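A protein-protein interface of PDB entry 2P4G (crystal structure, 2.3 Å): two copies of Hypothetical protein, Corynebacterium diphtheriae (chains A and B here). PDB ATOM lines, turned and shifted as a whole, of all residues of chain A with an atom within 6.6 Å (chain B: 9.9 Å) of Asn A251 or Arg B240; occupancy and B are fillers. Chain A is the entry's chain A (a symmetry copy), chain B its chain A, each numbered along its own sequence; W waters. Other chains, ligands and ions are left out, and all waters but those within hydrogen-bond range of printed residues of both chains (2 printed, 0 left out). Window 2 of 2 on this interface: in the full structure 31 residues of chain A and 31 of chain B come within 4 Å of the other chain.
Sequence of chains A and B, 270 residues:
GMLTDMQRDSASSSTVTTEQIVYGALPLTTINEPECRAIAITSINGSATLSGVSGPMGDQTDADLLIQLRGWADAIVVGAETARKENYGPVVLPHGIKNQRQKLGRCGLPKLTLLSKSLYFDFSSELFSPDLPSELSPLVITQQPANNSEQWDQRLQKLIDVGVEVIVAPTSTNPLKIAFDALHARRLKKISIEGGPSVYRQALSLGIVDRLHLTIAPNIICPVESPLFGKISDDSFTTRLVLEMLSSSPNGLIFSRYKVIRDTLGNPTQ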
ATOM      1  N   ASP A  59      11.334   2.109  -5.959  1.00  0.00           N
ATOM      2  CA  ASP A  59       9.897   2.358  -5.896  1.00  0.00           C
ATOM      3  C   ASP A  59       9.219   1.001  -5.713  1.00  0.00           C
ATOM      4  O   ASP A  59       9.887   0.011  -5.404  1.00  0.00           O
ATOM      5  CB  ASP A  59       9.388   3.129  -7.131  1.00  0.00           C
ATOM      6  CG  ASP A  59       9.522   2.341  -8.433  1.00  0.00           C
ATOM      7  OD1 ASP A  59      10.047   1.213  -8.424  1.00  0.00           O
ATOM      8  OD2 ASP A  59       9.109   2.870  -9.481  1.00  0.00           O
ATOM      9  N   GLN A  60       7.903   0.953  -5.886  1.00  0.00           N
ATOM     10  CA  GLN A  60       7.159  -0.270  -5.660  1.00  0.00           C
ATOM     11  C   GLN A  60       7.469  -1.316  -6.703  1.00  0.00           C
ATOM     12  O   GLN A  60       7.549  -2.480  -6.388  1.00  0.00           O
ATOM     13  CB  GLN A  60       5.646  -0.008  -5.642  1.00  0.00           C
ATOM     14  CG  GLN A  60       4.857  -1.199  -5.090  1.00  0.00           C
ATOM     15  CD  GLN A  60       5.387  -1.675  -3.739  1.00  0.00           C
ATOM     16  OE1 GLN A  60       5.400  -0.912  -2.773  1.00  0.00           O
ATOM     17  NE2 GLN A  60       5.839  -2.934  -3.671  1.00  0.00           N
ATOM     18  N   THR A  61       7.632  -0.901  -7.948  1.00  0.00           N
ATOM     19  CA  THR A  61       7.957  -1.843  -9.028  1.00  0.00           C
ATOM     20  C   THR A  61       9.241  -2.583  -8.672  1.00  0.00           C
ATOM     21  O   THR A  61       9.268  -3.803  -8.645  1.00  0.00           O
ATOM     22  CB  THR A  61       8.043  -1.129 -10.381  1.00  0.00           C
ATOM     23  OG1 THR A  61       6.789  -0.466 -10.651  1.00  0.00           O
ATOM     24  CG2 THR A  61       8.332  -2.113 -11.477  1.00  0.00           C
ATOM     25  N   PRO A 218      16.315   7.299 -11.082  1.00  0.00           N
ATOM     26  CA  PRO A 218      16.407   8.614 -11.681  1.00  0.00           C
ATOM     27  C   PRO A 218      17.032   9.633 -10.718  1.00  0.00           C
ATOM     28  O   PRO A 218      16.411  10.637 -10.372  1.00  0.00           O
ATOM     29  CB  PRO A 218      14.944   8.937 -11.974  1.00  0.00           C
ATOM     30  CG  PRO A 218      14.198   8.253 -10.858  1.00  0.00           C
ATOM     31  CD  PRO A 218      14.924   6.960 -10.704  1.00  0.00           C
ATOM     32  N   ASN A 219      18.250   9.376 -10.263  1.00  0.00           N
ATOM     33  CA  ASN A 219      18.956  10.369  -9.465  1.00  0.00           C
ATOM     34  C   ASN A 219      20.466  10.411  -9.659  1.00  0.00           C
ATOM     35  O   ASN A 219      21.078   9.474 -10.162  1.00  0.00           O
ATOM     36  CB  ASN A 219      18.555  10.306  -7.981  1.00  0.00           C
ATOM     37  CG  ASN A 219      18.413   8.912  -7.468  1.00  0.00           C
ATOM     38  OD1 ASN A 219      17.308   8.464  -7.114  1.00  0.00           O
ATOM     39  ND2 ASN A 219      19.528   8.201  -7.428  1.00  0.00           N
ATOM     40  N   ILE A 220      21.031  11.564  -9.325  1.00  0.00           N
ATOM     41  CA  ILE A 220      22.469  11.820  -9.392  1.00  0.00           C
ATOM     42  C   ILE A 220      22.938  12.026  -7.976  1.00  0.00           C
ATOM     43  O   ILE A 220      22.348  12.790  -7.265  1.00  0.00           O
ATOM     44  CB  ILE A 220      22.775  13.111 -10.146  1.00  0.00           C
ATOM     45  CG1 ILE A 220      22.341  12.978 -11.613  1.00  0.00           C
ATOM     46  CG2 ILE A 220      24.237  13.485  -9.965  1.00  0.00           C
ATOM     47  CD1 ILE A 220      22.651  14.175 -12.473  1.00  0.00           C
ATOM     48  N   SER A 248      10.986   0.229 -17.812  1.00  0.00           N
ATOM     49  CA  SER A 248      10.955   1.293 -16.801  1.00  0.00           C
ATOM     50  C   SER A 248       9.648   1.319 -15.998  1.00  0.00           C
ATOM     51  O   SER A 248       8.619   0.847 -16.469  1.00  0.00           O
ATOM     52  CB  SER A 248      11.187   2.661 -17.462  1.00  0.00           C
ATOM     53  OG  SER A 248      10.054   3.099 -18.195  1.00  0.00           O
ATOM     54  N   SER A 249       9.707   1.860 -14.780  1.00  0.00           N
ATOM     55  CA  SER A 249       8.518   2.096 -13.944  1.00  0.00           C
ATOM     56  C   SER A 249       7.914   3.468 -14.229  1.00  0.00           C
ATOM     57  O   SER A 249       8.541   4.292 -14.900  1.00  0.00           O
ATOM     58  CB  SER A 249       8.879   2.000 -12.459  1.00  0.00           C
ATOM     59  OG  SER A 249       9.690   3.071 -12.036  1.00  0.00           O
ATOM     60  N   PRO A 250       6.696   3.737 -13.716  1.00  0.00           N
ATOM     61  CA  PRO A 250       6.111   5.068 -13.930  1.00  0.00           C
ATOM     62  C   PRO A 250       6.843   6.181 -13.185  1.00  0.00           C
ATOM     63  O   PRO A 250       6.668   7.346 -13.517  1.00  0.00           O
ATOM     64  CB  PRO A 250       4.670   4.925 -13.414  1.00  0.00           C
ATOM     65  CG  PRO A 250       4.465   3.457 -13.170  1.00  0.00           C
ATOM     66  CD  PRO A 250       5.797   2.866 -12.935  1.00  0.00           C
ATOM     67  N   ASN A 251       7.644   5.814 -12.188  1.00  0.00           N
ATOM     68  CA  ASN A 251       8.537   6.748 -11.511  1.00  0.00           C
ATOM     69  C   ASN A 251       9.886   6.951 -12.216  1.00  0.00           C
ATOM     70  O   ASN A 251      10.743   7.657 -11.700  1.00  0.00           O
ATOM     71  CB  ASN A 251       8.767   6.278 -10.087  1.00  0.00           C
ATOM     72  CG  ASN A 251       7.479   6.217  -9.291  1.00  0.00           C
ATOM     73  OD1 ASN A 251       7.085   5.160  -8.815  1.00  0.00           O
ATOM     74  ND2 ASN A 251       6.809   7.352  -9.161  1.00  0.00           N
ATOM     75  N   GLY A 252      10.079   6.324 -13.370  1.00  0.00           N
ATOM     76  CA  GLY A 252      11.248   6.574 -14.198  1.00  0.00           C
ATOM     77  C   GLY A 252      12.464   5.756 -13.821  1.00  0.00           C
ATOM     78  O   GLY A 252      13.578   6.065 -14.255  1.00  0.00           O
ATOM     79  N   LEU A 253      12.265   4.702 -13.034  1.00  0.00           N
ATOM     80  CA  LEU A 253      13.343   3.780 -12.744  1.00  0.00           C
ATOM     81  C   LEU A 253      13.500   2.852 -13.931  1.00  0.00           C
ATOM     82  O   LEU A 253      12.504   2.424 -14.516  1.00  0.00           O
ATOM     83  CB  LEU A 253      13.068   2.960 -11.480  1.00  0.00           C
ATOM     84  CG  LEU A 253      13.308   3.628 -10.103  1.00  0.00           C
ATOM     85  CD1 LEU A 253      12.273   4.701  -9.842  1.00  0.00           C
ATOM     86  CD2 LEU A 253      13.319   2.555  -8.989  1.00  0.00           C
ATOM     87  N   LEU B 204      25.906  21.018 -13.575  1.00  0.00           N
ATOM     88  CA  LEU B 204      24.875  20.553 -12.656  1.00  0.00           C
ATOM     89  C   LEU B 204      24.810  21.406 -11.420  1.00  0.00           C
ATOM     90  O   LEU B 204      23.732  21.824 -11.018  1.00  0.00           O
ATOM     91  CB  LEU B 204      25.118  19.098 -12.249  1.00  0.00           C
ATOM     92  CG  LEU B 204      24.823  18.124 -13.390  1.00  0.00           C
ATOM     93  CD1 LEU B 204      25.465  16.742 -13.165  1.00  0.00           C
ATOM     94  CD2 LEU B 204      23.319  18.033 -13.573  1.00  0.00           C
ATOM     95  N   VAL B 209      21.799  22.781 -16.466  1.00  0.00           N
ATOM     96  CA  VAL B 209      21.444  21.630 -17.289  1.00  0.00           C
ATOM     97  C   VAL B 209      19.950  21.393 -17.161  1.00  0.00           C
ATOM     98  O   VAL B 209      19.440  21.202 -16.051  1.00  0.00           O
ATOM     99  CB  VAL B 209      22.255  20.385 -16.863  1.00  0.00           C
ATOM    100  CG1 VAL B 209      21.869  19.154 -17.708  1.00  0.00           C
ATOM    101  CG2 VAL B 209      23.770  20.680 -16.981  1.00  0.00           C
ATOM    102  N   ASP B 210      19.244  21.463 -18.286  1.00  0.00           N
ATOM    103  CA  ASP B 210      17.785  21.250 -18.324  1.00  0.00           C
ATOM    104  C   ASP B 210      17.428  19.795 -18.550  1.00  0.00           C
ATOM    105  O   ASP B 210      16.433  19.316 -18.043  1.00  0.00           O
ATOM    106  CB  ASP B 210      17.164  22.037 -19.469  1.00  0.00           C
ATOM    107  CG  ASP B 210      17.428  23.495 -19.358  1.00  0.00           C
ATOM    108  OD1 ASP B 210      16.987  24.051 -18.343  1.00  0.00           O
ATOM    109  OD2 ASP B 210      18.079  24.079 -20.257  1.00  0.00           O
ATOM    110  N   ARG B 211      18.223  19.130 -19.385  1.00  0.00           N
ATOM    111  CA  ARG B 211      18.017  17.725 -19.756  1.00  0.00           C
ATOM    112  C   ARG B 211      19.351  17.050 -19.908  1.00  0.00           C
ATOM    113  O   ARG B 211      20.339  17.701 -20.229  1.00  0.00           O
ATOM    114  CB  ARG B 211      17.315  17.570 -21.101  1.00  0.00           C
ATOM    115  CG  ARG B 211      15.876  17.612 -20.976  1.00  0.00           C
ATOM    116  CD  ARG B 211      15.142  17.347 -22.263  1.00  0.00           C
ATOM    117  NE  ARG B 211      13.740  17.519 -21.918  1.00  0.00           N
ATOM    118  CZ  ARG B 211      13.154  18.701 -21.747  1.00  0.00           C
ATOM    119  NH1 ARG B 211      13.804  19.839 -21.990  1.00  0.00           N
ATOM    120  NH2 ARG B 211      11.884  18.743 -21.388  1.00  0.00           N
ATOM    121  N   LEU B 212      19.319  15.732 -19.737  1.00  0.00           N
ATOM    122  CA  LEU B 212      20.471  14.871 -19.857  1.00  0.00           C
ATOM    123  C   LEU B 212      20.143  13.747 -20.826  1.00  0.00           C
ATOM    124  O   LEU B 212      19.118  13.097 -20.678  1.00  0.00           O
ATOM    125  CB  LEU B 212      20.800  14.295 -18.477  1.00  0.00           C
ATOM    126  CG  LEU B 212      21.907  13.262 -18.326  1.00  0.00           C
ATOM    127  CD1 LEU B 212      23.235  13.799 -18.821  1.00  0.00           C
ATOM    128  CD2 LEU B 212      21.952  12.866 -16.868  1.00  0.00           C
ATOM    129  N   PHE B 237      26.591  17.235  -4.175  1.00  0.00           N
ATOM    130  CA  PHE B 237      25.156  17.409  -4.400  1.00  0.00           C
ATOM    131  C   PHE B 237      24.455  16.170  -4.925  1.00  0.00           C
ATOM    132  O   PHE B 237      25.067  15.304  -5.552  1.00  0.00           O
ATOM    133  CB  PHE B 237      24.899  18.547  -5.384  1.00  0.00           C
ATOM    134  CG  PHE B 237      25.153  18.177  -6.805  1.00  0.00           C
ATOM    135  CD1 PHE B 237      24.149  17.589  -7.562  1.00  0.00           C
ATOM    136  CD2 PHE B 237      26.384  18.404  -7.372  1.00  0.00           C
ATOM    137  CE1 PHE B 237      24.356  17.227  -8.845  1.00  0.00           C
ATOM    138  CE2 PHE B 237      26.611  18.067  -8.652  1.00  0.00           C
ATOM    139  CZ  PHE B 237      25.598  17.465  -9.409  1.00  0.00           C
ATOM    140  N   THR B 238      23.149  16.129  -4.690  1.00  0.00           N
ATOM    141  CA  THR B 238      22.280  15.142  -5.310  1.00  0.00           C
ATOM    142  C   THR B 238      21.188  15.855  -6.101  1.00  0.00           C
ATOM    143  O   THR B 238      20.889  17.008  -5.838  1.00  0.00           O
ATOM    144  CB  THR B 238      21.616  14.269  -4.255  1.00  0.00           C
ATOM    145  OG1 THR B 238      20.670  15.060  -3.528  1.00  0.00           O
ATOM    146  CG2 THR B 238      22.655  13.697  -3.292  1.00  0.00           C
ATOM    147  N   THR B 239      20.598  15.177  -7.074  1.00  0.00           N
ATOM    148  CA  THR B 239      19.403  15.697  -7.723  1.00  0.00           C
ATOM    149  C   THR B 239      18.561  14.569  -8.259  1.00  0.00           C
ATOM    150  O   THR B 239      19.075  13.496  -8.533  1.00  0.00           O
ATOM    151  CB  THR B 239      19.720  16.683  -8.878  1.00  0.00           C
ATOM    152  OG1 THR B 239      18.487  17.148  -9.454  1.00  0.00           O
ATOM    153  CG2 THR B 239      20.558  16.048  -9.953  1.00  0.00           C
ATOM    154  N   ARG B 240      17.265  14.818  -8.405  1.00  0.00           N
ATOM    155  CA  ARG B 240      16.388  13.858  -9.036  1.00  0.00           C
ATOM    156  C   ARG B 240      16.050  14.239 -10.477  1.00  0.00           C
ATOM    157  O   ARG B 240      16.128  15.425 -10.903  1.00  0.00           O
ATOM    158  CB  ARG B 240      15.125  13.582  -8.206  1.00  0.00           C
ATOM    159  CG  ARG B 240      14.701  12.063  -8.224  1.00  0.00           C
ATOM    160  CD  ARG B 240      13.399  11.802  -7.493  1.00  0.00           C
ATOM    161  NE  ARG B 240      12.638  10.661  -8.026  1.00  0.00           N
ATOM    162  CZ  ARG B 240      11.919  10.669  -9.156  1.00  0.00           C
ATOM    163  NH1 ARG B 240      11.857  11.757  -9.926  1.00  0.00           N
ATOM    164  NH2 ARG B 240      11.260   9.571  -9.532  1.00  0.00           N
ATOM    165  N   LEU B 241      15.716  13.185 -11.222  1.00  0.00           N
ATOM    166  CA  LEU B 241      15.525  13.244 -12.651  1.00  0.00           C
ATOM    167  C   LEU B 241      14.145  12.728 -12.942  1.00  0.00           C
ATOM    168  O   LEU B 241      13.578  11.992 -12.125  1.00  0.00           O
ATOM    169  CB  LEU B 241      16.561  12.363 -13.328  1.00  0.00           C
ATOM    170  CG  LEU B 241      18.035  12.711 -13.090  1.00  0.00           C
ATOM    171  CD1 LEU B 241      18.982  11.673 -13.750  1.00  0.00           C
ATOM    172  CD2 LEU B 241      18.325  14.119 -13.619  1.00  0.00           C
ATOM    173  N   VAL B 242      13.579  13.175 -14.065  1.00  0.00           N
ATOM    174  CA  VAL B 242      12.352  12.603 -14.633  1.00  0.00           C
ATOM    175  C   VAL B 242      12.769  11.940 -15.932  1.00  0.00           C
ATOM    176  O   VAL B 242      13.282  12.606 -16.835  1.00  0.00           O
ATOM    177  CB  VAL B 242      11.263  13.674 -14.883  1.00  0.00           C
ATOM    178  CG1 VAL B 242      10.068  13.111 -15.701  1.00  0.00           C
ATOM    179  CG2 VAL B 242      10.780  14.235 -13.559  1.00  0.00           C
ATOM    180  N   LEU B 243      12.605  10.624 -15.995  1.00  0.00           N
ATOM    181  CA  LEU B 243      12.861   9.867 -17.210  1.00  0.00           C
ATOM    182  C   LEU B 243      11.799  10.253 -18.239  1.00  0.00           C
ATOM    183  O   LEU B 243      10.610  10.183 -17.963  1.00  0.00           O
ATOM    184  CB  LEU B 243      12.827   8.357 -16.934  1.00  0.00           C
ATOM    185  CG  LEU B 243      13.162   7.447 -18.125  1.00  0.00           C
ATOM    186  CD1 LEU B 243      14.599   7.667 -18.587  1.00  0.00           C
ATOM    187  CD2 LEU B 243      12.875   5.954 -17.801  1.00  0.00           C
ATOM    188  N   GLU B 244      12.247  10.682 -19.409  1.00  0.00           N
ATOM    189  CA  GLU B 244      11.352  11.088 -20.482  1.00  0.00           C
ATOM    190  C   GLU B 244      11.321  10.109 -21.655  1.00  0.00           C
ATOM    191  O   GLU B 244      10.284   9.939 -22.296  1.00  0.00           O
ATOM    192  CB  GLU B 244      11.777  12.444 -20.999  1.00  0.00           C
ATOM    193  CG  GLU B 244      11.526  13.602 -20.071  1.00  0.00           C
ATOM    194  CD  GLU B 244      11.993  14.918 -20.676  1.00  0.00           C
ATOM    195  OE1 GLU B 244      12.781  14.895 -21.642  1.00  0.00           O
ATOM    196  OE2 GLU B 244      11.578  15.973 -20.183  1.00  0.00           O
ATOM    197  N   TYR B 258      16.543  12.312 -19.642  1.00  0.00           N
ATOM    198  CA  TYR B 258      15.964  12.804 -18.390  1.00  0.00           C
ATOM    199  C   TYR B 258      15.831  14.312 -18.377  1.00  0.00           C
ATOM    200  O   TYR B 258      16.671  15.027 -18.922  1.00  0.00           O
ATOM    201  CB  TYR B 258      16.879  12.489 -17.225  1.00  0.00           C
ATOM    202  CG  TYR B 258      17.117  11.031 -16.938  1.00  0.00           C
ATOM    203  CD1 TYR B 258      16.263  10.317 -16.078  1.00  0.00           C
ATOM    204  CD2 TYR B 258      18.232  10.369 -17.471  1.00  0.00           C
ATOM    205  CE1 TYR B 258      16.502   8.970 -15.766  1.00  0.00           C
ATOM    206  CE2 TYR B 258      18.477   9.014 -17.176  1.00  0.00           C
ATOM    207  CZ  TYR B 258      17.617   8.333 -16.314  1.00  0.00           C
ATOM    208  OH  TYR B 258      17.862   7.020 -16.030  1.00  0.00           O
ATOM    209  N   LYS B 259      14.813  14.781 -17.669  1.00  0.00           N
ATOM    210  CA  LYS B 259      14.658  16.191 -17.358  1.00  0.00           C
ATOM    211  C   LYS B 259      15.285  16.433 -15.998  1.00  0.00           C
ATOM    212  O   LYS B 259      14.970  15.734 -15.037  1.00  0.00           O
ATOM    213  CB  LYS B 259      13.173  16.557 -17.348  1.00  0.00           C
ATOM    214  CG  LYS B 259      12.801  17.899 -16.694  1.00  0.00           C
ATOM    215  CD  LYS B 259      13.381  19.105 -17.427  1.00  0.00           C
ATOM    216  CE  LYS B 259      12.538  20.348 -17.217  1.00  0.00           C
ATOM    217  NZ  LYS B 259      11.117  20.170 -17.664  1.00  0.00           N
ATOM    218  N   VAL B 260      16.153  17.435 -15.909  1.00  0.00           N
ATOM    219  CA  VAL B 260      16.815  17.777 -14.646  1.00  0.00           C
ATOM    220  C   VAL B 260      15.943  18.672 -13.776  1.00  0.00           C
ATOM    221  O   VAL B 260      15.506  19.713 -14.210  1.00  0.00           O
ATOM    222  CB  VAL B 260      18.164  18.462 -14.889  1.00  0.00           C
ATOM    223  CG1 VAL B 260      18.765  18.930 -13.583  1.00  0.00           C
ATOM    224  CG2 VAL B 260      19.092  17.522 -15.612  1.00  0.00           C
ATOM    225  N   ILE B 261      15.704  18.265 -12.540  1.00  0.00           N
ATOM    226  CA  ILE B 261      14.757  18.991 -11.675  1.00  0.00           C
ATOM    227  C   ILE B 261      15.459  19.973 -10.718  1.00  0.00           C
ATOM    228  O   ILE B 261      16.259  19.582  -9.861  1.00  0.00           O
ATOM    229  CB  ILE B 261      13.881  18.015 -10.901  1.00  0.00           C
ATOM    230  CG1 ILE B 261      13.116  17.121 -11.887  1.00  0.00           C
ATOM    231  CG2 ILE B 261      12.923  18.770  -9.979  1.00  0.00           C
ATOM    232  CD1 ILE B 261      12.706  15.767 -11.299  1.00  0.00           C
ATOM    233  N   ARG B 262      15.120  21.250 -10.861  1.00  0.00           N
ATOM    234  CA  ARG B 262      15.807  22.340 -10.160  1.00  0.00           C
ATOM    235  C   ARG B 262      15.250  22.555  -8.758  1.00  0.00           C
ATOM    236  O   ARG B 262      14.037  22.468  -8.555  1.00  0.00           O
ATOM    237  CB  ARG B 262      15.647  23.647 -10.934  1.00  0.00           C
ATOM    238  CG  ARG B 262      15.785  23.505 -12.430  1.00  0.00           C
ATOM    239  CD  ARG B 262      17.121  22.883 -12.812  1.00  0.00           C
ATOM    240  NE  ARG B 262      17.422  23.131 -14.213  1.00  0.00           N
ATOM    241  CZ  ARG B 262      17.725  24.329 -14.707  1.00  0.00           C
ATOM    242  NH1 ARG B 262      17.782  25.406 -13.921  1.00  0.00           N
ATOM    243  NH2 ARG B 262      17.983  24.457 -15.997  1.00  0.00           N
ATOM    244  N   ASP B 263      16.143  22.850  -7.812  1.00  0.00           N
ATOM    245  CA  ASP B 263      15.781  23.123  -6.412  1.00  0.00           C
ATOM    246  C   ASP B 263      14.972  21.981  -5.775  1.00  0.00           C
ATOM    247  O   ASP B 263      15.099  20.815  -6.171  1.00  0.00           O
ATOM    248  CB  ASP B 263      15.013  24.456  -6.287  1.00  0.00           C
ATOM    249  CG  ASP B 263      15.870  25.674  -6.647  1.00  0.00           C
ATOM    250  OD1 ASP B 263      16.513  25.685  -7.727  1.00  0.00           O
ATOM    251  OD2 ASP B 263      15.888  26.630  -5.843  1.00  0.00           O
HETATM  252  O   HOH W   1       9.248   8.802 -15.585  1.00  0.00           O
HETATM  253  O   HOH W   2      16.310   6.173 -14.082  1.00  0.00           O
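O of Thr B239 sits at hydrogen-bond distance from N of Ile A220. The backbone carbonyl oxygen (O) of Asn A251 is in hydrogen-bond range of the guanidinium group (NH2) of Arg B240, 2.9 Å away. O of Pro A218 lies within hydrogen-bond range of N of Leu B241 (2.8 Å).
OG1 of Thr B239 is in hydrogen-bond range of O of Ile B261 (3.3 Å). The backbone carbonyl oxygen (O) of Arg B240 lies within hydrogen-bond range of the backbone NH (N) of Ile B261 (3.3 Å). The side-chain amide oxygen (OD1) of Asn A251 sits close to the side-chain carboxylate (OD2) of Asp A59 (3.1 Å). The side-chain hydroxyl (OG) of Ser A249 sits close to the backbone NH (N) of Asn A251 (3.4 Å).
Among the printed residues, pairs that only touch across the chains: Ile A220 with Thr B238 (3.1 Å), Pro A218 with Arg B240 (3.1 Å), Asn A219 with Thr B239 (3.3 Å), Gly A252 with Leu B243 (3.6 Å), Ser A248 with Leu B243 (3.7 Å), Ile A220 with Leu B204 (3.9 Å) and Ile A220 with Phe B237 (3.9 Å).
Asn A251 touches just one residue of chain B: Arg B240 (2.9 Å). Of chain B, only Arg B240 and Leu B241 come within 4 Å of Pro A218. No residue of chain B comes within 4 Å of Ser A249. No residue of chain B comes within 4 Å of Pro A250. Of the printed residues of chain A, Thr B238 touches Ile A220. Printed residues of chain A within 4 Å of Thr B239: Asn A219 (3.3 Å) and Ile A220 (2.9 Å). Of the printed residues of chain A, Leu B241 touches Pro A218. The nearest residue of chain B that does not touch Asn A251 is Leu B241 (5.2 Å). The nearest residue of chain A that does not touch Arg B240 is Asn A219 (4.2 Å).
Of the 12 printed residues of chain A, 6 touch a printed residue of chain B. Printed residues of chain B that touch a printed residue of chain A: Leu B204, Phe B237, Thr B238, Thr B239, Arg B240, Leu B241 and Leu B243. Hydrophobic or aromatic side chains of chain B that line the printed part of chain A: Leu B204, Phe B237, Leu B241 and Leu B243. Along chain B the printed residues that touch a printed residue of chain A span positions 204 to 243. Among the printed residues, no Asp or Glu carboxylate lies within 4 Å of a Lys or Arg side-chain nitrogen of the other chain.
No position is printed for both chains. Of the 10 pairs that touch across the chains among the printed residues, none has its exchanged pair printed and touching as well.
Water W2 lies within hydrogen-bond range of the side-chain hydroxyl of Tyr B258 (2.6 Å) and the backbone carbonyl oxygen of Gly A252 (2.7 Å). Water W1 lies within hydrogen-bond range of O of Leu B243 (3.1 Å) and N of Gly A252 (3.4 Å).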
